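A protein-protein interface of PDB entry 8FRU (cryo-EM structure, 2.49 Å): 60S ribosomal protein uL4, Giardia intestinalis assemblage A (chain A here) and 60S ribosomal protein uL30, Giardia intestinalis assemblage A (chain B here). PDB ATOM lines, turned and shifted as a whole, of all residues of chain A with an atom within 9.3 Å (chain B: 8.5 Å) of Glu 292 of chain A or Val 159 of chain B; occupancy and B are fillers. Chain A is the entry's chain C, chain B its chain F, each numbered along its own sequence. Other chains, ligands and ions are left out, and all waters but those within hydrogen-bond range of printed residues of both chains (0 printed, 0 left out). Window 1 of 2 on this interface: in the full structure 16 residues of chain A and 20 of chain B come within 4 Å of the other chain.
Glu 292 of chain A touches Pro 157 of chain B.
Val 159 of chain B touches Glu 292 of chain A (CG2 to OE1, 3.7 Å).
O of Arg 293 of chain A touches CG1 of Val 159 of chain B, at 3.9 Å.
O of Ile 143 of chain B touches NZ of Lys 294 of chain A, at 3.96 Å.
CB of Pro 157 of chain B touches CB of Lys 294 of chain A, 3.9 Å away.
Tyr 144 of chain B touches Pro 297 of chain A.
CB of Arg 306 of chain A touches O of Val 159 of chain B (3.7 Å).
Arg 306 of chain A touches Asn 161 of chain B (O to N, 3.96 Å).
Leu 307 of chain A touches Val 159 of chain B.
Leu 307 of chain A touches Asp 160 of chain B (CD1 to CA, 3.9 Å).
Of the 16 printed residues of chain B, 10 touch a printed residue of chain A.
Printed residues of chain B that touch a printed residue of chain A: Ile 143, Tyr 144, Gly 147, Phe 148, Pro 157, Ile 158, Val 159, Asp 160, Asn 161 and Leu 163.
Hydrophobic or aromatic side chains of chain B that line the printed part of chain A: Phe 148, Pro 157, Val 159 and Leu 163.
Of the 16 printed residues of chain A, 7 touch a printed residue of chain B.
Printed residues of chain A that touch a printed residue of chain B: Leu 289, Glu 292, Arg 293, Lys 294, Pro 297, Arg 306 and Leu 307.
Hydrophobic or aromatic side chains of chain A that line the printed part of chain B: Leu 289, Pro 297 and Leu 307.
Among the printed residues, Asp or Glu carboxylates within 4 Å of a Lys or Arg side-chain nitrogen of the other chain: Arg 306 of chain A with Asp 160 of chain B.
The backbone carbonyl oxygen (O) of Gly 147 of chain B lies within hydrogen-bond range of the backbone NH (N) of Ile 158 of chain B (3.3 Å).
The side-chain carboxylate (OE1) of Glu 292 of chain A is in salt-bridge range of the guanidinium group (NH2) of Arg 306 of chain A, 3.4 Å away.
The backbone carbonyl oxygen (O) of Pro 297 of chain A lies within hydrogen-bond range of the backbone NH (N) of Leu 304 of chain A (3.2 Å).
N of Asn 162 of chain B is in hydrogen-bond range of OD1 of Asp 160 of chain B, 2.9 Å away.
OD1 of Asn 161 of chain B is in hydrogen-bond range of N of Ala 176 of chain B.
OD1 of Asp 160 of chain B is in hydrogen-bond range of N of Leu 163 of chain B, at 3.4 Å.
The side-chain carboxylate (OD2) of Asp 160 of chain B lies within salt-bridge range of the guanidinium group (NH2) of Arg 306 of chain A (3.6 Å).
The backbone carbonyl oxygen (O) of Gly 147 of chain B sits at hydrogen-bond distance from the side-chain amino group (NZ) of Lys 294 of chain A (3.1 Å).
The backbone carbonyl oxygen (O) of Ile 158 of chain B is in hydrogen-bond range of the side-chain amino group (NZ) of Lys 294 of chain A, at 3.2 Å.
O of Leu 307 of chain A lies within hydrogen-bond range of ND2 of Asn 161 of chain B, 3.0 Å away.
The backbone carbonyl oxygen (O) of Tyr 144 of chain B sits at hydrogen-bond distance from the side-chain amino group (NZ) of Lys 294 of chain A (3.2 Å).
Ile 291 of chain A touches none of the printed residues of chain B.
Printed residues of chain B within 4 Å of Lys 294 of chain A: Ile 143, Tyr 144, Gly 147, Phe 148, Pro 157 and Ile 158.
Of the printed residues of chain A, Gly 147 of chain B touches Lys 294.
Of the printed residues of chain A, Ile 158 of chain B touches Lys 294.
Val 159 of chain B touches just these residues of chain A: Glu 292 (3.7 Å), Arg 293 (3.9 Å), Arg 306 (3.7 Å) and Leu 307 (3.1 Å).
Ile 164 of chain B touches none of the printed residues of chain A.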
ATOM      1  N   LEU A 289     -26.763  -8.633  25.147  1.00  0.00           N
ATOM      2  CA  LEU A 289     -25.662  -8.641  24.197  1.00  0.00           C
ATOM      3  C   LEU A 289     -24.470  -7.860  24.741  1.00  0.00           C
ATOM      4  O   LEU A 289     -24.619  -6.917  25.520  1.00  0.00           O
ATOM      5  CB  LEU A 289     -26.122  -8.043  22.869  1.00  0.00           C
ATOM      6  CG  LEU A 289     -25.249  -8.265  21.639  1.00  0.00           C
ATOM      7  CD1 LEU A 289     -25.356  -9.696  21.158  1.00  0.00           C
ATOM      8  CD2 LEU A 289     -25.641  -7.290  20.544  1.00  0.00           C
ATOM      9  N   VAL A 290     -23.274  -8.260  24.315  1.00  0.00           N
ATOM     10  CA  VAL A 290     -22.031  -7.605  24.713  1.00  0.00           C
ATOM     11  C   VAL A 290     -21.560  -6.722  23.566  1.00  0.00           C
ATOM     12  O   VAL A 290     -21.448  -7.184  22.424  1.00  0.00           O
ATOM     13  CB  VAL A 290     -20.950  -8.631  25.088  1.00  0.00           C
ATOM     14  CG1 VAL A 290     -19.780  -7.939  25.756  1.00  0.00           C
ATOM     15  CG2 VAL A 290     -21.527  -9.716  25.979  1.00  0.00           C
ATOM     16  N   ILE A 291     -21.276  -5.457  23.866  1.00  0.00           N
ATOM     17  CA  ILE A 291     -20.957  -4.459  22.852  1.00  0.00           C
ATOM     18  C   ILE A 291     -19.664  -3.761  23.237  1.00  0.00           C
ATOM     19  O   ILE A 291     -19.533  -3.267  24.362  1.00  0.00           O
ATOM     20  CB  ILE A 291     -22.099  -3.439  22.691  1.00  0.00           C
ATOM     21  CG1 ILE A 291     -23.393  -4.163  22.315  1.00  0.00           C
ATOM     22  CG2 ILE A 291     -21.737  -2.400  21.650  1.00  0.00           C
ATOM     23  CD1 ILE A 291     -24.644  -3.394  22.640  1.00  0.00           C
ATOM     24  N   GLU A 292     -18.719  -3.705  22.303  1.00  0.00           N
ATOM     25  CA  GLU A 292     -17.436  -3.062  22.534  1.00  0.00           C
ATOM     26  C   GLU A 292     -17.061  -2.221  21.323  1.00  0.00           C
ATOM     27  O   GLU A 292     -17.556  -2.435  20.216  1.00  0.00           O
ATOM     28  CB  GLU A 292     -16.339  -4.090  22.825  1.00  0.00           C
ATOM     29  CG  GLU A 292     -16.533  -4.870  24.107  1.00  0.00           C
ATOM     30  CD  GLU A 292     -16.307  -6.359  23.921  1.00  0.00           C
ATOM     31  OE1 GLU A 292     -16.475  -6.852  22.786  1.00  0.00           O
ATOM     32  OE2 GLU A 292     -15.960  -7.037  24.911  1.00  0.00           O
ATOM     33  N   ARG A 293     -16.173  -1.258  21.549  1.00  0.00           N
ATOM     34  CA  ARG A 293     -15.719  -0.370  20.489  1.00  0.00           C
ATOM     35  C   ARG A 293     -14.871  -1.116  19.465  1.00  0.00           C
ATOM     36  O   ARG A 293     -14.166  -2.073  19.786  1.00  0.00           O
ATOM     37  CB  ARG A 293     -14.910   0.783  21.076  1.00  0.00           C
ATOM     38  CG  ARG A 293     -15.484   1.346  22.355  1.00  0.00           C
ATOM     39  CD  ARG A 293     -16.507   2.422  22.069  1.00  0.00           C
ATOM     40  NE  ARG A 293     -15.977   3.448  21.180  1.00  0.00           N
ATOM     41  CZ  ARG A 293     -16.726   4.286  20.477  1.00  0.00           C
ATOM     42  NH1 ARG A 293     -18.048   4.245  20.535  1.00  0.00           N
ATOM     43  NH2 ARG A 293     -16.135   5.185  19.695  1.00  0.00           N
ATOM     44  N   LYS A 294     -14.932  -0.651  18.222  1.00  0.00           N
ATOM     45  CA  LYS A 294     -14.162  -1.255  17.145  1.00  0.00           C
ATOM     46  C   LYS A 294     -12.727  -0.751  17.176  1.00  0.00           C
ATOM     47  O   LYS A 294     -12.483   0.458  17.193  1.00  0.00           O
ATOM     48  CB  LYS A 294     -14.792  -0.940  15.791  1.00  0.00           C
ATOM     49  CG  LYS A 294     -13.992  -1.446  14.604  1.00  0.00           C
ATOM     50  CD  LYS A 294     -14.406  -2.854  14.228  1.00  0.00           C
ATOM     51  CE  LYS A 294     -13.566  -3.400  13.097  1.00  0.00           C
ATOM     52  NZ  LYS A 294     -13.989  -4.769  12.708  1.00  0.00           N
ATOM     53  N   VAL A 295     -11.777  -1.684  17.183  1.00  0.00           N
ATOM     54  CA  VAL A 295     -10.358  -1.368  17.146  1.00  0.00           C
ATOM     55  C   VAL A 295      -9.710  -2.223  16.068  1.00  0.00           C
ATOM     56  O   VAL A 295     -10.234  -3.267  15.673  1.00  0.00           O
ATOM     57  CB  VAL A 295      -9.674  -1.596  18.508  1.00  0.00           C
ATOM     58  CG1 VAL A 295     -10.244  -0.647  19.549  1.00  0.00           C
ATOM     59  CG2 VAL A 295      -9.838  -3.038  18.950  1.00  0.00           C
ATOM     60  N   ASP A 296      -8.558  -1.770  15.590  1.00  0.00           N
ATOM     61  CA  ASP A 296      -7.871  -2.474  14.515  1.00  0.00           C
ATOM     62  C   ASP A 296      -7.161  -3.698  15.072  1.00  0.00           C
ATOM     63  O   ASP A 296      -6.262  -3.553  15.908  1.00  0.00           O
ATOM     64  CB  ASP A 296      -6.874  -1.553  13.823  1.00  0.00           C
ATOM     65  CG  ASP A 296      -6.317  -2.152  12.544  1.00  0.00           C
ATOM     66  OD1 ASP A 296      -6.880  -3.151  12.055  1.00  0.00           O
ATOM     67  OD2 ASP A 296      -5.320  -1.618  12.019  1.00  0.00           O
ATOM     68  N   PRO A 297      -7.521  -4.910  14.643  1.00  0.00           N
ATOM     69  CA  PRO A 297      -6.857  -6.100  15.198  1.00  0.00           C
ATOM     70  C   PRO A 297      -5.362  -6.126  14.946  1.00  0.00           C
ATOM     71  O   PRO A 297      -4.604  -6.599  15.801  1.00  0.00           O
ATOM     72  CB  PRO A 297      -7.573  -7.260  14.490  1.00  0.00           C
ATOM     73  CG  PRO A 297      -8.845  -6.681  13.984  1.00  0.00           C
ATOM     74  CD  PRO A 297      -8.545  -5.263  13.649  1.00  0.00           C
ATOM     75  N   GLU A 302      -2.588  -8.883  20.912  1.00  0.00           N
ATOM     76  CA  GLU A 302      -3.732  -9.325  21.703  1.00  0.00           C
ATOM     77  C   GLU A 302      -5.031  -9.184  20.917  1.00  0.00           C
ATOM     78  O   GLU A 302      -5.858 -10.108  20.875  1.00  0.00           O
ATOM     79  CB  GLU A 302      -3.797  -8.525  23.003  1.00  0.00           C
ATOM     80  CG  GLU A 302      -4.748  -9.087  24.036  1.00  0.00           C
ATOM     81  CD  GLU A 302      -4.237 -10.371  24.642  1.00  0.00           C
ATOM     82  OE1 GLU A 302      -3.034 -10.655  24.486  1.00  0.00           O
ATOM     83  OE2 GLU A 302      -5.033 -11.092  25.277  1.00  0.00           O
ATOM     84  N   ALA A 303      -5.220  -8.032  20.272  1.00  0.00           N
ATOM     85  CA  ALA A 303      -6.407  -7.832  19.451  1.00  0.00           C
ATOM     86  C   ALA A 303      -6.462  -8.843  18.319  1.00  0.00           C
ATOM     87  O   ALA A 303      -7.525  -9.401  18.025  1.00  0.00           O
ATOM     88  CB  ALA A 303      -6.428  -6.407  18.905  1.00  0.00           C
ATOM     89  N   LEU A 304      -5.325  -9.099  17.671  1.00  0.00           N
ATOM     90  CA  LEU A 304      -5.297 -10.101  16.611  1.00  0.00           C
ATOM     91  C   LEU A 304      -5.626 -11.485  17.150  1.00  0.00           C
ATOM     92  O   LEU A 304      -6.376 -12.241  16.523  1.00  0.00           O
ATOM     93  CB  LEU A 304      -3.934 -10.101  15.927  1.00  0.00           C
ATOM     94  CG  LEU A 304      -3.956 -10.550  14.469  1.00  0.00           C
ATOM     95  CD1 LEU A 304      -5.290 -10.222  13.833  1.00  0.00           C
ATOM     96  CD2 LEU A 304      -2.826  -9.901  13.704  1.00  0.00           C
ATOM     97  N   ALA A 305      -5.073 -11.841  18.310  1.00  0.00           N
ATOM     98  CA  ALA A 305      -5.361 -13.147  18.888  1.00  0.00           C
ATOM     99  C   ALA A 305      -6.834 -13.290  19.228  1.00  0.00           C
ATOM    100  O   ALA A 305      -7.359 -14.405  19.255  1.00  0.00           O
ATOM    101  CB  ALA A 305      -4.505 -13.371  20.133  1.00  0.00           C
ATOM    102  N   ARG A 306      -7.511 -12.176  19.504  1.00  0.00           N
ATOM    103  CA  ARG A 306      -8.944 -12.248  19.769  1.00  0.00           C
ATOM    104  C   ARG A 306      -9.727 -12.748  18.557  1.00  0.00           C
ATOM    105  O   ARG A 306     -10.815 -13.309  18.716  1.00  0.00           O
ATOM    106  CB  ARG A 306      -9.461 -10.882  20.216  1.00  0.00           C
ATOM    107  CG  ARG A 306      -9.882 -10.837  21.670  1.00  0.00           C
ATOM    108  CD  ARG A 306      -9.932  -9.417  22.196  1.00  0.00           C
ATOM    109  NE  ARG A 306     -11.246  -8.801  22.056  1.00  0.00           N
ATOM    110  CZ  ARG A 306     -12.313  -9.143  22.765  1.00  0.00           C
ATOM    111  NH1 ARG A 306     -12.270 -10.127  23.647  1.00  0.00           N
ATOM    112  NH2 ARG A 306     -13.451  -8.483  22.583  1.00  0.00           N
ATOM    113  N   LEU A 307      -9.196 -12.564  17.346  1.00  0.00           N
ATOM    114  CA  LEU A 307      -9.882 -12.968  16.122  1.00  0.00           C
ATOM    115  C   LEU A 307      -9.315 -14.234  15.490  1.00  0.00           C
ATOM    116  O   LEU A 307     -10.081 -15.043  14.962  1.00  0.00           O
ATOM    117  CB  LEU A 307      -9.848 -11.839  15.086  1.00  0.00           C
ATOM    118  CG  LEU A 307     -11.117 -11.007  14.865  1.00  0.00           C
ATOM    119  CD1 LEU A 307     -12.376 -11.829  15.083  1.00  0.00           C
ATOM    120  CD2 LEU A 307     -11.125  -9.767  15.735  1.00  0.00           C
ATOM    121  N   ASP A 308      -7.994 -14.428  15.507  1.00  0.00           N
ATOM    122  CA  ASP A 308      -7.379 -15.661  15.012  1.00  0.00           C
ATOM    123  C   ASP A 308      -6.457 -16.228  16.083  1.00  0.00           C
ATOM    124  O   ASP A 308      -5.281 -15.851  16.174  1.00  0.00           O
ATOM    125  CB  ASP A 308      -6.626 -15.432  13.703  1.00  0.00           C
ATOM    126  CG  ASP A 308      -5.576 -14.351  13.813  1.00  0.00           C
ATOM    127  OD1 ASP A 308      -5.915 -13.228  14.242  1.00  0.00           O
ATOM    128  OD2 ASP A 308      -4.407 -14.627  13.476  1.00  0.00           O
ATOM    129  N   ILE B 143     -13.068  -7.649   6.311  1.00  0.00           N
ATOM    130  CA  ILE B 143     -13.821  -8.120   7.466  1.00  0.00           C
ATOM    131  C   ILE B 143     -13.108  -7.765   8.767  1.00  0.00           C
ATOM    132  O   ILE B 143     -13.752  -7.408   9.759  1.00  0.00           O
ATOM    133  CB  ILE B 143     -14.092  -9.628   7.349  1.00  0.00           C
ATOM    134  CG1 ILE B 143     -15.287  -9.869   6.422  1.00  0.00           C
ATOM    135  CG2 ILE B 143     -14.334 -10.231   8.719  1.00  0.00           C
ATOM    136  CD1 ILE B 143     -15.703 -11.307   6.322  1.00  0.00           C
ATOM    137  N   TYR B 144     -11.779  -7.860   8.798  1.00  0.00           N
ATOM    138  CA  TYR B 144     -11.062  -7.601  10.043  1.00  0.00           C
ATOM    139  C   TYR B 144     -11.057  -6.120  10.392  1.00  0.00           C
ATOM    140  O   TYR B 144     -11.191  -5.756  11.564  1.00  0.00           O
ATOM    141  CB  TYR B 144      -9.630  -8.126   9.951  1.00  0.00           C
ATOM    142  CG  TYR B 144      -9.492  -9.598  10.255  1.00  0.00           C
ATOM    143  CD1 TYR B 144     -10.514 -10.484   9.969  1.00  0.00           C
ATOM    144  CD2 TYR B 144      -8.336 -10.101  10.828  1.00  0.00           C
ATOM    145  CE1 TYR B 144     -10.392 -11.824  10.239  1.00  0.00           C
ATOM    146  CE2 TYR B 144      -8.203 -11.444  11.104  1.00  0.00           C
ATOM    147  CZ  TYR B 144      -9.236 -12.300  10.808  1.00  0.00           C
ATOM    148  OH  TYR B 144      -9.110 -13.641  11.082  1.00  0.00           O
ATOM    149  N   GLY B 147     -15.386  -4.592   9.646  1.00  0.00           N
ATOM    150  CA  GLY B 147     -16.495  -5.508   9.803  1.00  0.00           C
ATOM    151  C   GLY B 147     -17.449  -5.169  10.928  1.00  0.00           C
ATOM    152  O   GLY B 147     -17.040  -5.027  12.081  1.00  0.00           O
ATOM    153  N   PHE B 148     -18.728  -5.036  10.597  1.00  0.00           N
ATOM    154  CA  PHE B 148     -19.783  -4.794  11.566  1.00  0.00           C
ATOM    155  C   PHE B 148     -20.934  -5.743  11.277  1.00  0.00           C
ATOM    156  O   PHE B 148     -21.148  -6.149  10.134  1.00  0.00           O
ATOM    157  CB  PHE B 148     -20.285  -3.340  11.526  1.00  0.00           C
ATOM    158  CG  PHE B 148     -19.296  -2.337  12.029  1.00  0.00           C
ATOM    159  CD1 PHE B 148     -18.211  -1.967  11.259  1.00  0.00           C
ATOM    160  CD2 PHE B 148     -19.452  -1.758  13.271  1.00  0.00           C
ATOM    161  CE1 PHE B 148     -17.303  -1.049  11.719  1.00  0.00           C
ATOM    162  CE2 PHE B 148     -18.547  -0.837  13.732  1.00  0.00           C
ATOM    163  CZ  PHE B 148     -17.470  -0.482  12.954  1.00  0.00           C
ATOM    164  N   ALA B 149     -21.680  -6.086  12.318  1.00  0.00           N
ATOM    165  CA  ALA B 149     -22.769  -7.045  12.219  1.00  0.00           C
ATOM    166  C   ALA B 149     -24.109  -6.348  12.394  1.00  0.00           C
ATOM    167  O   ALA B 149     -24.228  -5.400  13.171  1.00  0.00           O
ATOM    168  CB  ALA B 149     -22.625  -8.149  13.265  1.00  0.00           C
ATOM    169  N   ARG B 155     -25.996  -1.804  14.576  1.00  0.00           N
ATOM    170  CA  ARG B 155     -24.698  -2.012  13.931  1.00  0.00           C
ATOM    171  C   ARG B 155     -23.667  -2.315  15.014  1.00  0.00           C
ATOM    172  O   ARG B 155     -23.170  -1.407  15.681  1.00  0.00           O
ATOM    173  CB  ARG B 155     -24.295  -0.799  13.098  1.00  0.00           C
ATOM    174  CG  ARG B 155     -23.187  -1.101  12.110  1.00  0.00           C
ATOM    175  CD  ARG B 155     -22.961   0.010  11.113  1.00  0.00           C
ATOM    176  NE  ARG B 155     -21.969   0.963  11.581  1.00  0.00           N
ATOM    177  CZ  ARG B 155     -20.786   1.151  11.020  1.00  0.00           C
ATOM    178  NH1 ARG B 155     -20.421   0.490   9.941  1.00  0.00           N
ATOM    179  NH2 ARG B 155     -19.948   2.030  11.555  1.00  0.00           N
ATOM    180  N   ILE B 156     -23.335  -3.587  15.172  1.00  0.00           N
ATOM    181  CA  ILE B 156     -22.493  -4.061  16.270  1.00  0.00           C
ATOM    182  C   ILE B 156     -21.096  -4.350  15.732  1.00  0.00           C
ATOM    183  O   ILE B 156     -20.971  -5.058  14.725  1.00  0.00           O
ATOM    184  CB  ILE B 156     -23.089  -5.314  16.931  1.00  0.00           C
ATOM    185  CG1 ILE B 156     -24.588  -5.132  17.173  1.00  0.00           C
ATOM    186  CG2 ILE B 156     -22.377  -5.617  18.227  1.00  0.00           C
ATOM    187  CD1 ILE B 156     -24.930  -3.998  18.102  1.00  0.00           C
ATOM    188  N   PRO B 157     -20.042  -3.832  16.354  1.00  0.00           N
ATOM    189  CA  PRO B 157     -18.687  -4.131  15.880  1.00  0.00           C
ATOM    190  C   PRO B 157     -18.322  -5.592  16.077  1.00  0.00           C
ATOM    191  O   PRO B 157     -18.747  -6.241  17.033  1.00  0.00           O
ATOM    192  CB  PRO B 157     -17.804  -3.222  16.743  1.00  0.00           C
ATOM    193  CG  PRO B 157     -18.725  -2.171  17.258  1.00  0.00           C
ATOM    194  CD  PRO B 157     -20.026  -2.874  17.468  1.00  0.00           C
ATOM    195  N   ILE B 158     -17.500  -6.099  15.164  1.00  0.00           N
ATOM    196  CA  ILE B 158     -16.969  -7.453  15.236  1.00  0.00           C
ATOM    197  C   ILE B 158     -15.528  -7.379  15.724  1.00  0.00           C
ATOM    198  O   ILE B 158     -14.649  -6.880  15.013  1.00  0.00           O
ATOM    199  CB  ILE B 158     -17.050  -8.162  13.875  1.00  0.00           C
ATOM    200  CG1 ILE B 158     -18.498  -8.231  13.388  1.00  0.00           C
ATOM    201  CG2 ILE B 158     -16.439  -9.544  13.957  1.00  0.00           C
ATOM    202  CD1 ILE B 158     -18.635  -8.727  11.979  1.00  0.00           C
ATOM    203  N   VAL B 159     -15.278  -7.890  16.930  1.00  0.00           N
ATOM    204  CA  VAL B 159     -13.943  -7.891  17.513  1.00  0.00           C
ATOM    205  C   VAL B 159     -13.530  -9.252  18.050  1.00  0.00           C
ATOM    206  O   VAL B 159     -12.399  -9.403  18.506  1.00  0.00           O
ATOM    207  CB  VAL B 159     -13.813  -6.829  18.625  1.00  0.00           C
ATOM    208  CG1 VAL B 159     -13.390  -5.489  18.041  1.00  0.00           C
ATOM    209  CG2 VAL B 159     -15.118  -6.694  19.383  1.00  0.00           C
ATOM    210  N   ASP B 160     -14.411 -10.248  18.020  1.00  0.00           N
ATOM    211  CA  ASP B 160     -14.092 -11.570  18.541  1.00  0.00           C
ATOM    212  C   ASP B 160     -15.051 -12.594  17.954  1.00  0.00           C
ATOM    213  O   ASP B 160     -16.098 -12.246  17.403  1.00  0.00           O
ATOM    214  CB  ASP B 160     -14.099 -11.571  20.077  1.00  0.00           C
ATOM    215  CG  ASP B 160     -15.500 -11.644  20.682  1.00  0.00           C
ATOM    216  OD1 ASP B 160     -16.476 -12.003  19.995  1.00  0.00           O
ATOM    217  OD2 ASP B 160     -15.620 -11.326  21.883  1.00  0.00           O
ATOM    218  N   ASN B 161     -14.682 -13.866  18.088  1.00  0.00           N
ATOM    219  CA  ASN B 161     -15.415 -14.956  17.458  1.00  0.00           C
ATOM    220  C   ASN B 161     -16.676 -15.357  18.207  1.00  0.00           C
ATOM    221  O   ASN B 161     -17.466 -16.137  17.670  1.00  0.00           O
ATOM    222  CB  ASN B 161     -14.513 -16.182  17.318  1.00  0.00           C
ATOM    223  CG  ASN B 161     -13.466 -16.015  16.247  1.00  0.00           C
ATOM    224  OD1 ASN B 161     -13.758 -15.563  15.144  1.00  0.00           O
ATOM    225  ND2 ASN B 161     -12.232 -16.374  16.568  1.00  0.00           N
ATOM    226  N   ASN B 162     -16.880 -14.861  19.426  1.00  0.00           N
ATOM    227  CA  ASN B 162     -18.075 -15.231  20.176  1.00  0.00           C
ATOM    228  C   ASN B 162     -19.341 -14.736  19.490  1.00  0.00           C
ATOM    229  O   ASN B 162     -20.343 -15.454  19.429  1.00  0.00           O
ATOM    230  CB  ASN B 162     -17.984 -14.688  21.600  1.00  0.00           C
ATOM    231  CG  ASN B 162     -16.744 -15.165  22.317  1.00  0.00           C
ATOM    232  OD1 ASN B 162     -15.956 -15.930  21.767  1.00  0.00           O
ATOM    233  ND2 ASN B 162     -16.565 -14.721  23.552  1.00  0.00           N
ATOM    234  N   LEU B 163     -19.316 -13.511  18.969  1.00  0.00           N
ATOM    235  CA  LEU B 163     -20.498 -12.952  18.324  1.00  0.00           C
ATOM    236  C   LEU B 163     -20.887 -13.761  17.094  1.00  0.00           C
ATOM    237  O   LEU B 163     -22.061 -14.109  16.905  1.00  0.00           O
ATOM    238  CB  LEU B 163     -20.236 -11.495  17.950  1.00  0.00           C
ATOM    239  CG  LEU B 163     -21.435 -10.648  17.533  1.00  0.00           C
ATOM    240  CD1 LEU B 163     -22.279 -10.306  18.739  1.00  0.00           C
ATOM    241  CD2 LEU B 163     -20.961  -9.394  16.830  1.00  0.00           C
ATOM    242  N   ILE B 164     -19.907 -14.067  16.243  1.00  0.00           N
ATOM    243  CA  ILE B 164     -20.176 -14.850  15.043  1.00  0.00           C
ATOM    244  C   ILE B 164     -20.785 -16.192  15.418  1.00  0.00           C
ATOM    245  O   ILE B 164     -21.788 -16.625  14.842  1.00  0.00           O
ATOM    246  CB  ILE B 164     -18.886 -15.026  14.223  1.00  0.00           C
ATOM    247  CG1 ILE B 164     -18.133 -13.702  14.139  1.00  0.00           C
ATOM    248  CG2 ILE B 164     -19.195 -15.556  12.840  1.00  0.00           C
ATOM    249  CD1 ILE B 164     -16.720 -13.834  13.622  1.00  0.00           C
ATOM    250  N   ALA B 176     -14.173 -16.329  12.488  1.00  0.00           N
ATOM    251  CA  ALA B 176     -13.894 -15.475  11.341  1.00  0.00           C
ATOM    252  C   ALA B 176     -13.402 -16.275  10.143  1.00  0.00           C
ATOM    253  O   ALA B 176     -13.707 -15.922   8.997  1.00  0.00           O
ATOM    254  CB  ALA B 176     -12.874 -14.408  11.726  1.00  0.00           C
